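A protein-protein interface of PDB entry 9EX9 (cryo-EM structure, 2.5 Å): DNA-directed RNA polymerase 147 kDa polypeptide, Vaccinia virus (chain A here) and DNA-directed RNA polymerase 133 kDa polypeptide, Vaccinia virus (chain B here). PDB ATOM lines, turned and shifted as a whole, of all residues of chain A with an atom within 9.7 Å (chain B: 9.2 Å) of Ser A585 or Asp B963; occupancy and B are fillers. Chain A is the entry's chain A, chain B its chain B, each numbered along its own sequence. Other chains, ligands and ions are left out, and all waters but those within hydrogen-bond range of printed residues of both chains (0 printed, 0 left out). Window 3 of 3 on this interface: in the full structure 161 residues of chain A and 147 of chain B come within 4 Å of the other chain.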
ATOM      1  N   PHE A 578     -24.819 -28.186 -24.600  1.00  0.00           N
ATOM      2  CA  PHE A 578     -24.327 -26.879 -25.020  1.00  0.00           C
ATOM      3  C   PHE A 578     -24.438 -25.854 -23.902  1.00  0.00           C
ATOM      4  O   PHE A 578     -23.586 -24.969 -23.789  1.00  0.00           O
ATOM      5  CB  PHE A 578     -25.093 -26.408 -26.255  1.00  0.00           C
ATOM      6  CG  PHE A 578     -24.576 -25.126 -26.840  1.00  0.00           C
ATOM      7  CD1 PHE A 578     -23.299 -25.053 -27.362  1.00  0.00           C
ATOM      8  CD2 PHE A 578     -25.373 -23.998 -26.882  1.00  0.00           C
ATOM      9  CE1 PHE A 578     -22.823 -23.878 -27.902  1.00  0.00           C
ATOM     10  CE2 PHE A 578     -24.901 -22.823 -27.423  1.00  0.00           C
ATOM     11  CZ  PHE A 578     -23.625 -22.763 -27.934  1.00  0.00           C
ATOM     12  N   LEU A 581     -21.351 -25.321 -21.809  1.00  0.00           N
ATOM     13  CA  LEU A 581     -20.218 -24.603 -22.374  1.00  0.00           C
ATOM     14  C   LEU A 581     -20.467 -23.106 -22.477  1.00  0.00           C
ATOM     15  O   LEU A 581     -19.550 -22.314 -22.249  1.00  0.00           O
ATOM     16  CB  LEU A 581     -19.891 -25.165 -23.758  1.00  0.00           C
ATOM     17  CG  LEU A 581     -18.776 -24.488 -24.552  1.00  0.00           C
ATOM     18  CD1 LEU A 581     -17.431 -24.784 -23.933  1.00  0.00           C
ATOM     19  CD2 LEU A 581     -18.814 -24.938 -25.995  1.00  0.00           C
ATOM     20  N   ARG A 582     -21.685 -22.697 -22.819  1.00  0.00           N
ATOM     21  CA  ARG A 582     -21.990 -21.289 -23.070  1.00  0.00           C
ATOM     22  C   ARG A 582     -23.422 -21.003 -22.652  1.00  0.00           C
ATOM     23  O   ARG A 582     -24.325 -20.897 -23.489  1.00  0.00           O
ATOM     24  CB  ARG A 582     -21.774 -20.941 -24.542  1.00  0.00           C
ATOM     25  CG  ARG A 582     -21.884 -19.466 -24.858  1.00  0.00           C
ATOM     26  CD  ARG A 582     -21.522 -19.192 -26.298  1.00  0.00           C
ATOM     27  NE  ARG A 582     -21.619 -17.779 -26.634  1.00  0.00           N
ATOM     28  CZ  ARG A 582     -22.743 -17.161 -26.970  1.00  0.00           C
ATOM     29  NH1 ARG A 582     -23.902 -17.795 -26.989  1.00  0.00           N
ATOM     30  NH2 ARG A 582     -22.703 -15.873 -27.288  1.00  0.00           N
ATOM     31  N   PRO A 583     -23.671 -20.875 -21.347  1.00  0.00           N
ATOM     32  CA  PRO A 583     -25.041 -20.574 -20.897  1.00  0.00           C
ATOM     33  C   PRO A 583     -25.579 -19.269 -21.448  1.00  0.00           C
ATOM     34  O   PRO A 583     -26.777 -19.162 -21.735  1.00  0.00           O
ATOM     35  CB  PRO A 583     -24.903 -20.526 -19.372  1.00  0.00           C
ATOM     36  CG  PRO A 583     -23.625 -21.211 -19.065  1.00  0.00           C
ATOM     37  CD  PRO A 583     -22.731 -20.981 -20.223  1.00  0.00           C
ATOM     38  N   ASN A 584     -24.723 -18.266 -21.592  1.00  0.00           N
ATOM     39  CA  ASN A 584     -25.106 -16.965 -22.119  1.00  0.00           C
ATOM     40  C   ASN A 584     -23.848 -16.306 -22.670  1.00  0.00           C
ATOM     41  O   ASN A 584     -22.786 -16.931 -22.746  1.00  0.00           O
ATOM     42  CB  ASN A 584     -25.789 -16.122 -21.039  1.00  0.00           C
ATOM     43  CG  ASN A 584     -25.043 -16.147 -19.733  1.00  0.00           C
ATOM     44  OD1 ASN A 584     -23.916 -15.675 -19.645  1.00  0.00           O
ATOM     45  ND2 ASN A 584     -25.670 -16.698 -18.706  1.00  0.00           N
ATOM     46  N   SER A 585     -23.959 -15.032 -23.040  1.00  0.00           N
ATOM     47  CA  SER A 585     -22.903 -14.334 -23.761  1.00  0.00           C
ATOM     48  C   SER A 585     -22.192 -13.289 -22.909  1.00  0.00           C
ATOM     49  O   SER A 585     -21.701 -12.294 -23.446  1.00  0.00           O
ATOM     50  CB  SER A 585     -23.482 -13.683 -25.015  1.00  0.00           C
ATOM     51  OG  SER A 585     -24.552 -12.818 -24.689  1.00  0.00           O
ATOM     52  N   THR A 586     -22.114 -13.490 -21.595  1.00  0.00           N
ATOM     53  CA  THR A 586     -21.459 -12.509 -20.736  1.00  0.00           C
ATOM     54  C   THR A 586     -19.943 -12.686 -20.742  1.00  0.00           C
ATOM     55  O   THR A 586     -19.197 -11.759 -21.079  1.00  0.00           O
ATOM     56  CB  THR A 586     -22.007 -12.621 -19.313  1.00  0.00           C
ATOM     57  OG1 THR A 586     -23.415 -12.364 -19.321  1.00  0.00           O
ATOM     58  CG2 THR A 586     -21.325 -11.629 -18.394  1.00  0.00           C
ATOM     59  N   PHE A 587     -19.472 -13.876 -20.373  1.00  0.00           N
ATOM     60  CA  PHE A 587     -18.036 -14.099 -20.265  1.00  0.00           C
ATOM     61  C   PHE A 587     -17.347 -13.939 -21.613  1.00  0.00           C
ATOM     62  O   PHE A 587     -16.267 -13.340 -21.702  1.00  0.00           O
ATOM     63  CB  PHE A 587     -17.769 -15.486 -19.688  1.00  0.00           C
ATOM     64  CG  PHE A 587     -16.321 -15.857 -19.665  1.00  0.00           C
ATOM     65  CD1 PHE A 587     -15.448 -15.217 -18.814  1.00  0.00           C
ATOM     66  CD2 PHE A 587     -15.833 -16.843 -20.494  1.00  0.00           C
ATOM     67  CE1 PHE A 587     -14.118 -15.552 -18.792  1.00  0.00           C
ATOM     68  CE2 PHE A 587     -14.502 -17.182 -20.474  1.00  0.00           C
ATOM     69  CZ  PHE A 587     -13.645 -16.535 -19.623  1.00  0.00           C
ATOM     70  N   THR A 588     -17.947 -14.478 -22.673  1.00  0.00           N
ATOM     71  CA  THR A 588     -17.329 -14.377 -23.989  1.00  0.00           C
ATOM     72  C   THR A 588     -17.219 -12.925 -24.432  1.00  0.00           C
ATOM     73  O   THR A 588     -16.185 -12.511 -24.965  1.00  0.00           O
ATOM     74  CB  THR A 588     -18.120 -15.193 -25.010  1.00  0.00           C
ATOM     75  OG1 THR A 588     -19.520 -14.942 -24.845  1.00  0.00           O
ATOM     76  CG2 THR A 588     -17.850 -16.670 -24.835  1.00  0.00           C
ATOM     77  N   ASN A 589     -18.271 -12.135 -24.221  1.00  0.00           N
ATOM     78  CA  ASN A 589     -18.211 -10.727 -24.593  1.00  0.00           C
ATOM     79  C   ASN A 589     -17.148  -9.990 -23.792  1.00  0.00           C
ATOM     80  O   ASN A 589     -16.408  -9.160 -24.337  1.00  0.00           O
ATOM     81  CB  ASN A 589     -19.576 -10.076 -24.395  1.00  0.00           C
ATOM     82  CG  ASN A 589     -20.589 -10.543 -25.406  1.00  0.00           C
ATOM     83  OD1 ASN A 589     -20.239 -11.163 -26.404  1.00  0.00           O
ATOM     84  ND2 ASN A 589     -21.853 -10.239 -25.161  1.00  0.00           N
ATOM     85  N   LYS A 590     -17.057 -10.277 -22.494  1.00  0.00           N
ATOM     86  CA  LYS A 590     -16.041  -9.631 -21.672  1.00  0.00           C
ATOM     87  C   LYS A 590     -14.644  -9.922 -22.207  1.00  0.00           C
ATOM     88  O   LYS A 590     -13.834  -9.007 -22.418  1.00  0.00           O
ATOM     89  CB  LYS A 590     -16.177 -10.108 -20.228  1.00  0.00           C
ATOM     90  CG  LYS A 590     -15.330  -9.344 -19.241  1.00  0.00           C
ATOM     91  CD  LYS A 590     -15.253 -10.051 -17.905  1.00  0.00           C
ATOM     92  CE  LYS A 590     -14.378 -11.284 -17.983  1.00  0.00           C
ATOM     93  NZ  LYS A 590     -14.123 -11.857 -16.639  1.00  0.00           N
ATOM     94  N   LEU A 591     -14.349 -11.197 -22.447  1.00  0.00           N
ATOM     95  CA  LEU A 591     -13.016 -11.564 -22.909  1.00  0.00           C
ATOM     96  C   LEU A 591     -12.737 -10.993 -24.296  1.00  0.00           C
ATOM     97  O   LEU A 591     -11.606 -10.586 -24.596  1.00  0.00           O
ATOM     98  CB  LEU A 591     -12.874 -13.083 -22.895  1.00  0.00           C
ATOM     99  CG  LEU A 591     -11.472 -13.676 -22.975  1.00  0.00           C
ATOM    100  CD1 LEU A 591     -10.523 -12.993 -22.014  1.00  0.00           C
ATOM    101  CD2 LEU A 591     -11.541 -15.154 -22.675  1.00  0.00           C
ATOM    102  N   GLU A 592     -13.759 -10.938 -25.151  1.00  0.00           N
ATOM    103  CA  GLU A 592     -13.591 -10.360 -26.477  1.00  0.00           C
ATOM    104  C   GLU A 592     -13.224  -8.886 -26.393  1.00  0.00           C
ATOM    105  O   GLU A 592     -12.323  -8.420 -27.101  1.00  0.00           O
ATOM    106  CB  GLU A 592     -14.873 -10.550 -27.281  1.00  0.00           C
ATOM    107  CG  GLU A 592     -14.857  -9.903 -28.642  1.00  0.00           C
ATOM    108  CD  GLU A 592     -16.143 -10.134 -29.402  1.00  0.00           C
ATOM    109  OE1 GLU A 592     -16.938 -10.998 -28.980  1.00  0.00           O
ATOM    110  OE2 GLU A 592     -16.363  -9.446 -30.421  1.00  0.00           O
ATOM    111  N   ALA A 593     -13.913  -8.131 -25.537  1.00  0.00           N
ATOM    112  CA  ALA A 593     -13.581  -6.720 -25.385  1.00  0.00           C
ATOM    113  C   ALA A 593     -12.168  -6.546 -24.847  1.00  0.00           C
ATOM    114  O   ALA A 593     -11.430  -5.649 -25.282  1.00  0.00           O
ATOM    115  CB  ALA A 593     -14.592  -6.040 -24.467  1.00  0.00           C
ATOM    116  N   HIS A 648     -12.455 -18.169 -14.577  1.00  0.00           N
ATOM    117  CA  HIS A 648     -13.834 -18.487 -14.929  1.00  0.00           C
ATOM    118  C   HIS A 648     -14.179 -19.921 -14.557  1.00  0.00           C
ATOM    119  O   HIS A 648     -15.281 -20.192 -14.068  1.00  0.00           O
ATOM    120  CB  HIS A 648     -14.058 -18.253 -16.419  1.00  0.00           C
ATOM    121  CG  HIS A 648     -15.431 -18.619 -16.886  1.00  0.00           C
ATOM    122  ND1 HIS A 648     -15.659 -19.593 -17.832  1.00  0.00           N
ATOM    123  CD2 HIS A 648     -16.647 -18.138 -16.541  1.00  0.00           C
ATOM    124  CE1 HIS A 648     -16.957 -19.696 -18.052  1.00  0.00           C
ATOM    125  NE2 HIS A 648     -17.578 -18.823 -17.280  1.00  0.00           N
ATOM    126  N   LEU A 680     -13.182 -20.628 -26.238  1.00  0.00           N
ATOM    127  CA  LEU A 680     -13.841 -19.429 -25.736  1.00  0.00           C
ATOM    128  C   LEU A 680     -12.949 -18.200 -25.686  1.00  0.00           C
ATOM    129  O   LEU A 680     -13.474 -17.090 -25.591  1.00  0.00           O
ATOM    130  CB  LEU A 680     -14.379 -19.672 -24.319  1.00  0.00           C
ATOM    131  CG  LEU A 680     -15.423 -20.770 -24.123  1.00  0.00           C
ATOM    132  CD1 LEU A 680     -15.483 -21.181 -22.671  1.00  0.00           C
ATOM    133  CD2 LEU A 680     -16.779 -20.298 -24.590  1.00  0.00           C
ATOM    134  N   THR A 723     -15.891 -20.186 -30.946  1.00  0.00           N
ATOM    135  CA  THR A 723     -17.281 -19.775 -30.775  1.00  0.00           C
ATOM    136  C   THR A 723     -17.589 -18.527 -31.590  1.00  0.00           C
ATOM    137  O   THR A 723     -18.680 -18.397 -32.155  1.00  0.00           O
ATOM    138  CB  THR A 723     -17.585 -19.529 -29.299  1.00  0.00           C
ATOM    139  OG1 THR A 723     -16.595 -18.658 -28.743  1.00  0.00           O
ATOM    140  CG2 THR A 723     -17.594 -20.830 -28.532  1.00  0.00           C
ATOM    141  N   LYS A 724     -16.649 -17.586 -31.638  1.00  0.00           N
ATOM    142  CA  LYS A 724     -16.827 -16.396 -32.459  1.00  0.00           C
ATOM    143  C   LYS A 724     -16.775 -16.745 -33.940  1.00  0.00           C
ATOM    144  O   LYS A 724     -17.635 -16.324 -34.719  1.00  0.00           O
ATOM    145  CB  LYS A 724     -15.754 -15.370 -32.100  1.00  0.00           C
ATOM    146  CG  LYS A 724     -15.644 -14.185 -33.032  1.00  0.00           C
ATOM    147  CD  LYS A 724     -16.882 -13.334 -33.016  1.00  0.00           C
ATOM    148  CE  LYS A 724     -16.619 -12.001 -33.680  1.00  0.00           C
ATOM    149  NZ  LYS A 724     -17.799 -11.104 -33.615  1.00  0.00           N
ATOM    150  N   HIS B 681     -15.864 -22.735 -37.342  1.00  0.00           N
ATOM    151  CA  HIS B 681     -16.042 -22.895 -35.906  1.00  0.00           C
ATOM    152  C   HIS B 681     -15.399 -24.165 -35.362  1.00  0.00           C
ATOM    153  O   HIS B 681     -15.567 -24.459 -34.177  1.00  0.00           O
ATOM    154  CB  HIS B 681     -17.527 -22.912 -35.550  1.00  0.00           C
ATOM    155  CG  HIS B 681     -18.253 -21.652 -35.893  1.00  0.00           C
ATOM    156  ND1 HIS B 681     -18.206 -20.528 -35.101  1.00  0.00           N
ATOM    157  CD2 HIS B 681     -19.068 -21.350 -36.927  1.00  0.00           C
ATOM    158  CE1 HIS B 681     -18.951 -19.581 -35.641  1.00  0.00           C
ATOM    159  NE2 HIS B 681     -19.487 -20.055 -36.750  1.00  0.00           N
ATOM    160  N   ILE B 930     -24.754 -26.283 -33.136  1.00  0.00           N
ATOM    161  CA  ILE B 930     -25.557 -25.235 -33.752  1.00  0.00           C
ATOM    162  C   ILE B 930     -26.467 -25.839 -34.804  1.00  0.00           C
ATOM    163  O   ILE B 930     -27.667 -25.546 -34.849  1.00  0.00           O
ATOM    164  CB  ILE B 930     -24.649 -24.147 -34.350  1.00  0.00           C
ATOM    165  CG1 ILE B 930     -23.781 -23.517 -33.264  1.00  0.00           C
ATOM    166  CG2 ILE B 930     -25.487 -23.091 -35.038  1.00  0.00           C
ATOM    167  CD1 ILE B 930     -22.628 -22.718 -33.812  1.00  0.00           C
ATOM    168  N   LEU B 934     -30.568 -25.290 -35.180  1.00  0.00           N
ATOM    169  CA  LEU B 934     -31.239 -24.697 -36.326  1.00  0.00           C
ATOM    170  C   LEU B 934     -32.220 -25.681 -36.932  1.00  0.00           C
ATOM    171  O   LEU B 934     -33.366 -25.322 -37.228  1.00  0.00           O
ATOM    172  CB  LEU B 934     -30.212 -24.241 -37.358  1.00  0.00           C
ATOM    173  CG  LEU B 934     -29.311 -23.104 -36.882  1.00  0.00           C
ATOM    174  CD1 LEU B 934     -28.232 -22.820 -37.897  1.00  0.00           C
ATOM    175  CD2 LEU B 934     -30.129 -21.861 -36.609  1.00  0.00           C
ATOM    176  N   ASN B 958     -19.106 -19.168 -41.635  1.00  0.00           N
ATOM    177  CA  ASN B 958     -20.406 -18.643 -41.231  1.00  0.00           C
ATOM    178  C   ASN B 958     -20.467 -17.122 -41.306  1.00  0.00           C
ATOM    179  O   ASN B 958     -21.154 -16.560 -42.165  1.00  0.00           O
ATOM    180  CB  ASN B 958     -20.721 -19.114 -39.813  1.00  0.00           C
ATOM    181  CG  ASN B 958     -21.889 -18.389 -39.218  1.00  0.00           C
ATOM    182  OD1 ASN B 958     -22.872 -18.122 -39.900  1.00  0.00           O
ATOM    183  ND2 ASN B 958     -21.786 -18.047 -37.941  1.00  0.00           N
ATOM    184  N   THR B 960     -21.962 -15.178 -39.257  1.00  0.00           N
ATOM    185  CA  THR B 960     -23.109 -14.726 -38.481  1.00  0.00           C
ATOM    186  C   THR B 960     -22.922 -15.090 -37.014  1.00  0.00           C
ATOM    187  O   THR B 960     -22.237 -16.058 -36.678  1.00  0.00           O
ATOM    188  CB  THR B 960     -24.406 -15.351 -39.001  1.00  0.00           C
ATOM    189  OG1 THR B 960     -24.656 -14.912 -40.339  1.00  0.00           O
ATOM    190  CG2 THR B 960     -25.579 -14.972 -38.126  1.00  0.00           C
ATOM    191  N   SER B 961     -23.549 -14.306 -36.143  1.00  0.00           N
ATOM    192  CA  SER B 961     -23.387 -14.470 -34.707  1.00  0.00           C
ATOM    193  C   SER B 961     -24.311 -15.552 -34.165  1.00  0.00           C
ATOM    194  O   SER B 961     -25.414 -15.771 -34.670  1.00  0.00           O
ATOM    195  CB  SER B 961     -23.672 -13.151 -33.992  1.00  0.00           C
ATOM    196  OG  SER B 961     -23.407 -13.257 -32.610  1.00  0.00           O
ATOM    197  N   ILE B 962     -23.848 -16.229 -33.115  1.00  0.00           N
ATOM    198  CA  ILE B 962     -24.654 -17.267 -32.482  1.00  0.00           C
ATOM    199  C   ILE B 962     -25.902 -16.666 -31.850  1.00  0.00           C
ATOM    200  O   ILE B 962     -26.972 -17.285 -31.846  1.00  0.00           O
ATOM    201  CB  ILE B 962     -23.814 -18.036 -31.448  1.00  0.00           C
ATOM    202  CG1 ILE B 962     -22.787 -18.918 -32.159  1.00  0.00           C
ATOM    203  CG2 ILE B 962     -24.720 -18.862 -30.553  1.00  0.00           C
ATOM    204  CD1 ILE B 962     -21.883 -19.695 -31.230  1.00  0.00           C
ATOM    205  N   ASP B 963     -25.788 -15.457 -31.302  1.00  0.00           N
ATOM    206  CA  ASP B 963     -26.937 -14.830 -30.663  1.00  0.00           C
ATOM    207  C   ASP B 963     -28.068 -14.604 -31.655  1.00  0.00           C
ATOM    208  O   ASP B 963     -29.244 -14.760 -31.311  1.00  0.00           O
ATOM    209  CB  ASP B 963     -26.518 -13.513 -30.022  1.00  0.00           C
ATOM    210  CG  ASP B 963     -25.448 -13.697 -28.975  1.00  0.00           C
ATOM    211  OD1 ASP B 963     -25.471 -14.733 -28.279  1.00  0.00           O
ATOM    212  OD2 ASP B 963     -24.580 -12.811 -28.848  1.00  0.00           O
ATOM    213  N   THR B 964     -27.735 -14.227 -32.889  1.00  0.00           N
ATOM    214  CA  THR B 964     -28.768 -14.032 -33.900  1.00  0.00           C
ATOM    215  C   THR B 964     -29.478 -15.340 -34.222  1.00  0.00           C
ATOM    216  O   THR B 964     -30.700 -15.368 -34.402  1.00  0.00           O
ATOM    217  CB  THR B 964     -28.158 -13.430 -35.162  1.00  0.00           C
ATOM    218  OG1 THR B 964     -27.522 -12.189 -34.840  1.00  0.00           O
ATOM    219  CG2 THR B 964     -29.229 -13.181 -36.202  1.00  0.00           C
ATOM    220  N   TYR B 965     -28.726 -16.436 -34.302  1.00  0.00           N
ATOM    221  CA  TYR B 965     -29.343 -17.740 -34.517  1.00  0.00           C
ATOM    222  C   TYR B 965     -30.267 -18.108 -33.366  1.00  0.00           C
ATOM    223  O   TYR B 965     -31.370 -18.627 -33.582  1.00  0.00           O
ATOM    224  CB  TYR B 965     -28.259 -18.799 -34.689  1.00  0.00           C
ATOM    225  CG  TYR B 965     -27.573 -18.796 -36.036  1.00  0.00           C
ATOM    226  CD1 TYR B 965     -28.275 -18.524 -37.199  1.00  0.00           C
ATOM    227  CD2 TYR B 965     -26.223 -19.074 -36.143  1.00  0.00           C
ATOM    228  CE1 TYR B 965     -27.652 -18.528 -38.420  1.00  0.00           C
ATOM    229  CE2 TYR B 965     -25.595 -19.079 -37.360  1.00  0.00           C
ATOM    230  CZ  TYR B 965     -26.315 -18.806 -38.495  1.00  0.00           C
ATOM    231  OH  TYR B 965     -25.683 -18.813 -39.713  1.00  0.00           O
ATOM    232  N   MET B 966     -29.835 -17.849 -32.132  1.00  0.00           N
ATOM    233  CA  MET B 966     -30.690 -18.123 -30.985  1.00  0.00           C
ATOM    234  C   MET B 966     -31.959 -17.284 -31.037  1.00  0.00           C
ATOM    235  O   MET B 966     -33.043 -17.764 -30.693  1.00  0.00           O
ATOM    236  CB  MET B 966     -29.930 -17.851 -29.694  1.00  0.00           C
ATOM    237  CG  MET B 966     -28.719 -18.729 -29.484  1.00  0.00           C
ATOM    238  SD  MET B 966     -29.138 -20.425 -29.088  1.00  0.00           S
ATOM    239  CE  MET B 966     -27.537 -21.029 -28.581  1.00  0.00           C
ATOM    240  N   GLN B 967     -31.846 -16.025 -31.456  1.00  0.00           N
ATOM    241  CA  GLN B 967     -33.033 -15.183 -31.562  1.00  0.00           C
ATOM    242  C   GLN B 967     -33.990 -15.713 -32.623  1.00  0.00           C
ATOM    243  O   GLN B 967     -35.210 -15.723 -32.424  1.00  0.00           O
ATOM    244  CB  GLN B 967     -32.623 -13.748 -31.875  1.00  0.00           C
ATOM    245  CG  GLN B 967     -33.776 -12.765 -31.881  1.00  0.00           C
ATOM    246  CD  GLN B 967     -34.478 -12.691 -30.544  1.00  0.00           C
ATOM    247  OE1 GLN B 967     -33.889 -12.979 -29.505  1.00  0.00           O
ATOM    248  NE2 GLN B 967     -35.749 -12.312 -30.564  1.00  0.00           N
ATOM    249  N   PHE B 968     -33.453 -16.159 -33.756  1.00  0.00           N
ATOM    250  CA  PHE B 968     -34.297 -16.741 -34.795  1.00  0.00           C
ATOM    251  C   PHE B 968     -35.027 -17.978 -34.281  1.00  0.00           C
ATOM    252  O   PHE B 968     -36.237 -18.132 -34.492  1.00  0.00           O
ATOM    253  CB  PHE B 968     -33.434 -17.075 -36.011  1.00  0.00           C
ATOM    254  CG  PHE B 968     -34.104 -17.964 -37.013  1.00  0.00           C
ATOM    255  CD1 PHE B 968     -35.120 -17.484 -37.817  1.00  0.00           C
ATOM    256  CD2 PHE B 968     -33.703 -19.276 -37.164  1.00  0.00           C
ATOM    257  CE1 PHE B 968     -35.727 -18.299 -38.737  1.00  0.00           C
ATOM    258  CE2 PHE B 968     -34.309 -20.091 -38.083  1.00  0.00           C
ATOM    259  CZ  PHE B 968     -35.323 -19.602 -38.870  1.00  0.00           C
ATOM    260  N   ALA B 969     -34.307 -18.862 -33.585  1.00  0.00           N
ATOM    261  CA  ALA B 969     -34.933 -20.055 -33.022  1.00  0.00           C
ATOM    262  C   ALA B 969     -36.013 -19.692 -32.013  1.00  0.00           C
ATOM    263  O   ALA B 969     -37.089 -20.307 -31.986  1.00  0.00           O
ATOM    264  CB  ALA B 969     -33.872 -20.936 -32.371  1.00  0.00           C
ATOM    265  N   LYS B 970     -35.739 -18.703 -31.163  1.00  0.00           N
ATOM    266  CA  LYS B 970     -36.729 -18.266 -30.189  1.00  0.00           C
ATOM    267  C   LYS B 970     -37.986 -17.764 -30.878  1.00  0.00           C
ATOM    268  O   LYS B 970     -39.102 -18.067 -30.444  1.00  0.00           O
ATOM    269  CB  LYS B 970     -36.134 -17.174 -29.306  1.00  0.00           C
ATOM    270  CG  LYS B 970     -37.117 -16.541 -28.353  1.00  0.00           C
ATOM    271  CD  LYS B 970     -36.422 -15.577 -27.421  1.00  0.00           C
ATOM    272  CE  LYS B 970     -37.412 -14.893 -26.503  1.00  0.00           C
ATOM    273  NZ  LYS B 970     -36.749 -13.946 -25.572  1.00  0.00           N
ATOM    274  N   GLN B 971     -37.827 -16.985 -31.946  1.00  0.00           N
ATOM    275  CA  GLN B 971     -38.998 -16.507 -32.671  1.00  0.00           C
ATOM    276  C   GLN B 971     -39.784 -17.665 -33.265  1.00  0.00           C
ATOM    277  O   GLN B 971     -41.020 -17.668 -33.231  1.00  0.00           O
ATOM    278  CB  GLN B 971     -38.577 -15.536 -33.769  1.00  0.00           C
ATOM    279  CG  GLN B 971     -38.113 -14.194 -33.259  1.00  0.00           C
ATOM    280  CD  GLN B 971     -37.628 -13.299 -34.375  1.00  0.00           C
ATOM    281  OE1 GLN B 971     -37.903 -13.550 -35.548  1.00  0.00           O
ATOM    282  NE2 GLN B 971     -36.896 -12.252 -34.019  1.00  0.00           N
ATOM    283  N   ILE B 989     -34.982 -23.997 -26.924  1.00  0.00           N
ATOM    284  CA  ILE B 989     -33.953 -23.303 -27.692  1.00  0.00           C
ATOM    285  C   ILE B 989     -32.628 -24.041 -27.602  1.00  0.00           C
ATOM    286  O   ILE B 989     -31.925 -24.200 -28.604  1.00  0.00           O
ATOM    287  CB  ILE B 989     -33.813 -21.847 -27.219  1.00  0.00           C
ATOM    288  CG1 ILE B 989     -35.021 -21.029 -27.666  1.00  0.00           C
ATOM    289  CG2 ILE B 989     -32.532 -21.247 -27.760  1.00  0.00           C
ATOM    290  CD1 ILE B 989     -35.081 -19.657 -27.051  1.00  0.00           C
ATOM    291  N   PHE B 990     -32.256 -24.493 -26.410  1.00  0.00           N
ATOM    292  CA  PHE B 990     -30.994 -25.198 -26.241  1.00  0.00           C
ATOM    293  C   PHE B 990     -31.100 -26.689 -26.529  1.00  0.00           C
ATOM    294  O   PHE B 990     -30.087 -27.388 -26.445  1.00  0.00           O
ATOM    295  CB  PHE B 990     -30.461 -24.987 -24.827  1.00  0.00           C
ATOM    296  CG  PHE B 990     -29.737 -23.691 -24.645  1.00  0.00           C
ATOM    297  CD1 PHE B 990     -28.384 -23.598 -24.906  1.00  0.00           C
ATOM    298  CD2 PHE B 990     -30.406 -22.566 -24.210  1.00  0.00           C
ATOM    299  CE1 PHE B 990     -27.717 -22.412 -24.737  1.00  0.00           C
ATOM    300  CE2 PHE B 990     -29.740 -21.378 -24.042  1.00  0.00           C
ATOM    301  CZ  PHE B 990     -28.395 -21.302 -24.305  1.00  0.00           C
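Printed residues of chain A that touch a printed residue of chain B: Phe A578, Arg A582, Pro A583, Ser A585, Thr A723 and Lys A724. Hydrophobic or aromatic side chains of chain A that line the printed part of chain B: Phe A578. Printed residues of chain B that touch a printed residue of chain A: His B681, Ile B962, Asp B963, Met B966 and Phe B990. Among the printed residues, 10 pairs touch across the chains.
OD1 of Asp B963 is in salt-bridge range of NH2 of Arg A582.
O of Ser A585 sits at hydrogen-bond distance from ND2 of Asn A589 (2.7 Å). The side-chain carboxylate (OE2) of Glu A592 lies within salt-bridge range of the side-chain amino group (NZ) of Lys A724, at 3.9 Å. NE2 of His B681 lies within hydrogen-bond range of ND2 of Asn B958, at 3.3 Å. The side-chain hydroxyl (OG) of Ser B961 sits close to the backbone NH (N) of Asp B963, 3.5 Å away.
Among the printed residues, pairs that only touch across the chains: Phe A578 with Met B966 (3.4 Å), Phe A578 with Phe B990 (3.6 Å), Arg A582 with Ile B962 (3.8 Å), Arg A582 with Phe B990 (3.9 Å), Pro A583 with Phe B990 (3.7 Å), Ser A585 with Asp B963 (3.96 Å), Thr A723 with His B681 (3.7 Å), Thr A723 with Ile B962 (3.6 Å) and Lys A724 with His B681 (3.6 Å).
Ser A585 touches one residue of chain B. No residue of chain B comes within 4 Å of Thr A586. Thr B964 touches none of the printed residues of chain A. Printed residues of chain B within 4 Å of Lys A724: His B681. Of the printed residues of chain A, Ile B962 touches Arg A582 and Thr A723. Printed residues of chain A within 4 Å of Phe B990: Phe A578, Arg A582 and Pro A583. Asn A589 touches none of the printed residues of chain B. Phe A587 touches none of the printed residues of chain B. The nearest residue of chain B that does not touch Ser A585 is Ser B961 (7.6 Å). The nearest residue of chain A that does not touch Asp B963 is Asn A589 (5.2 Å).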
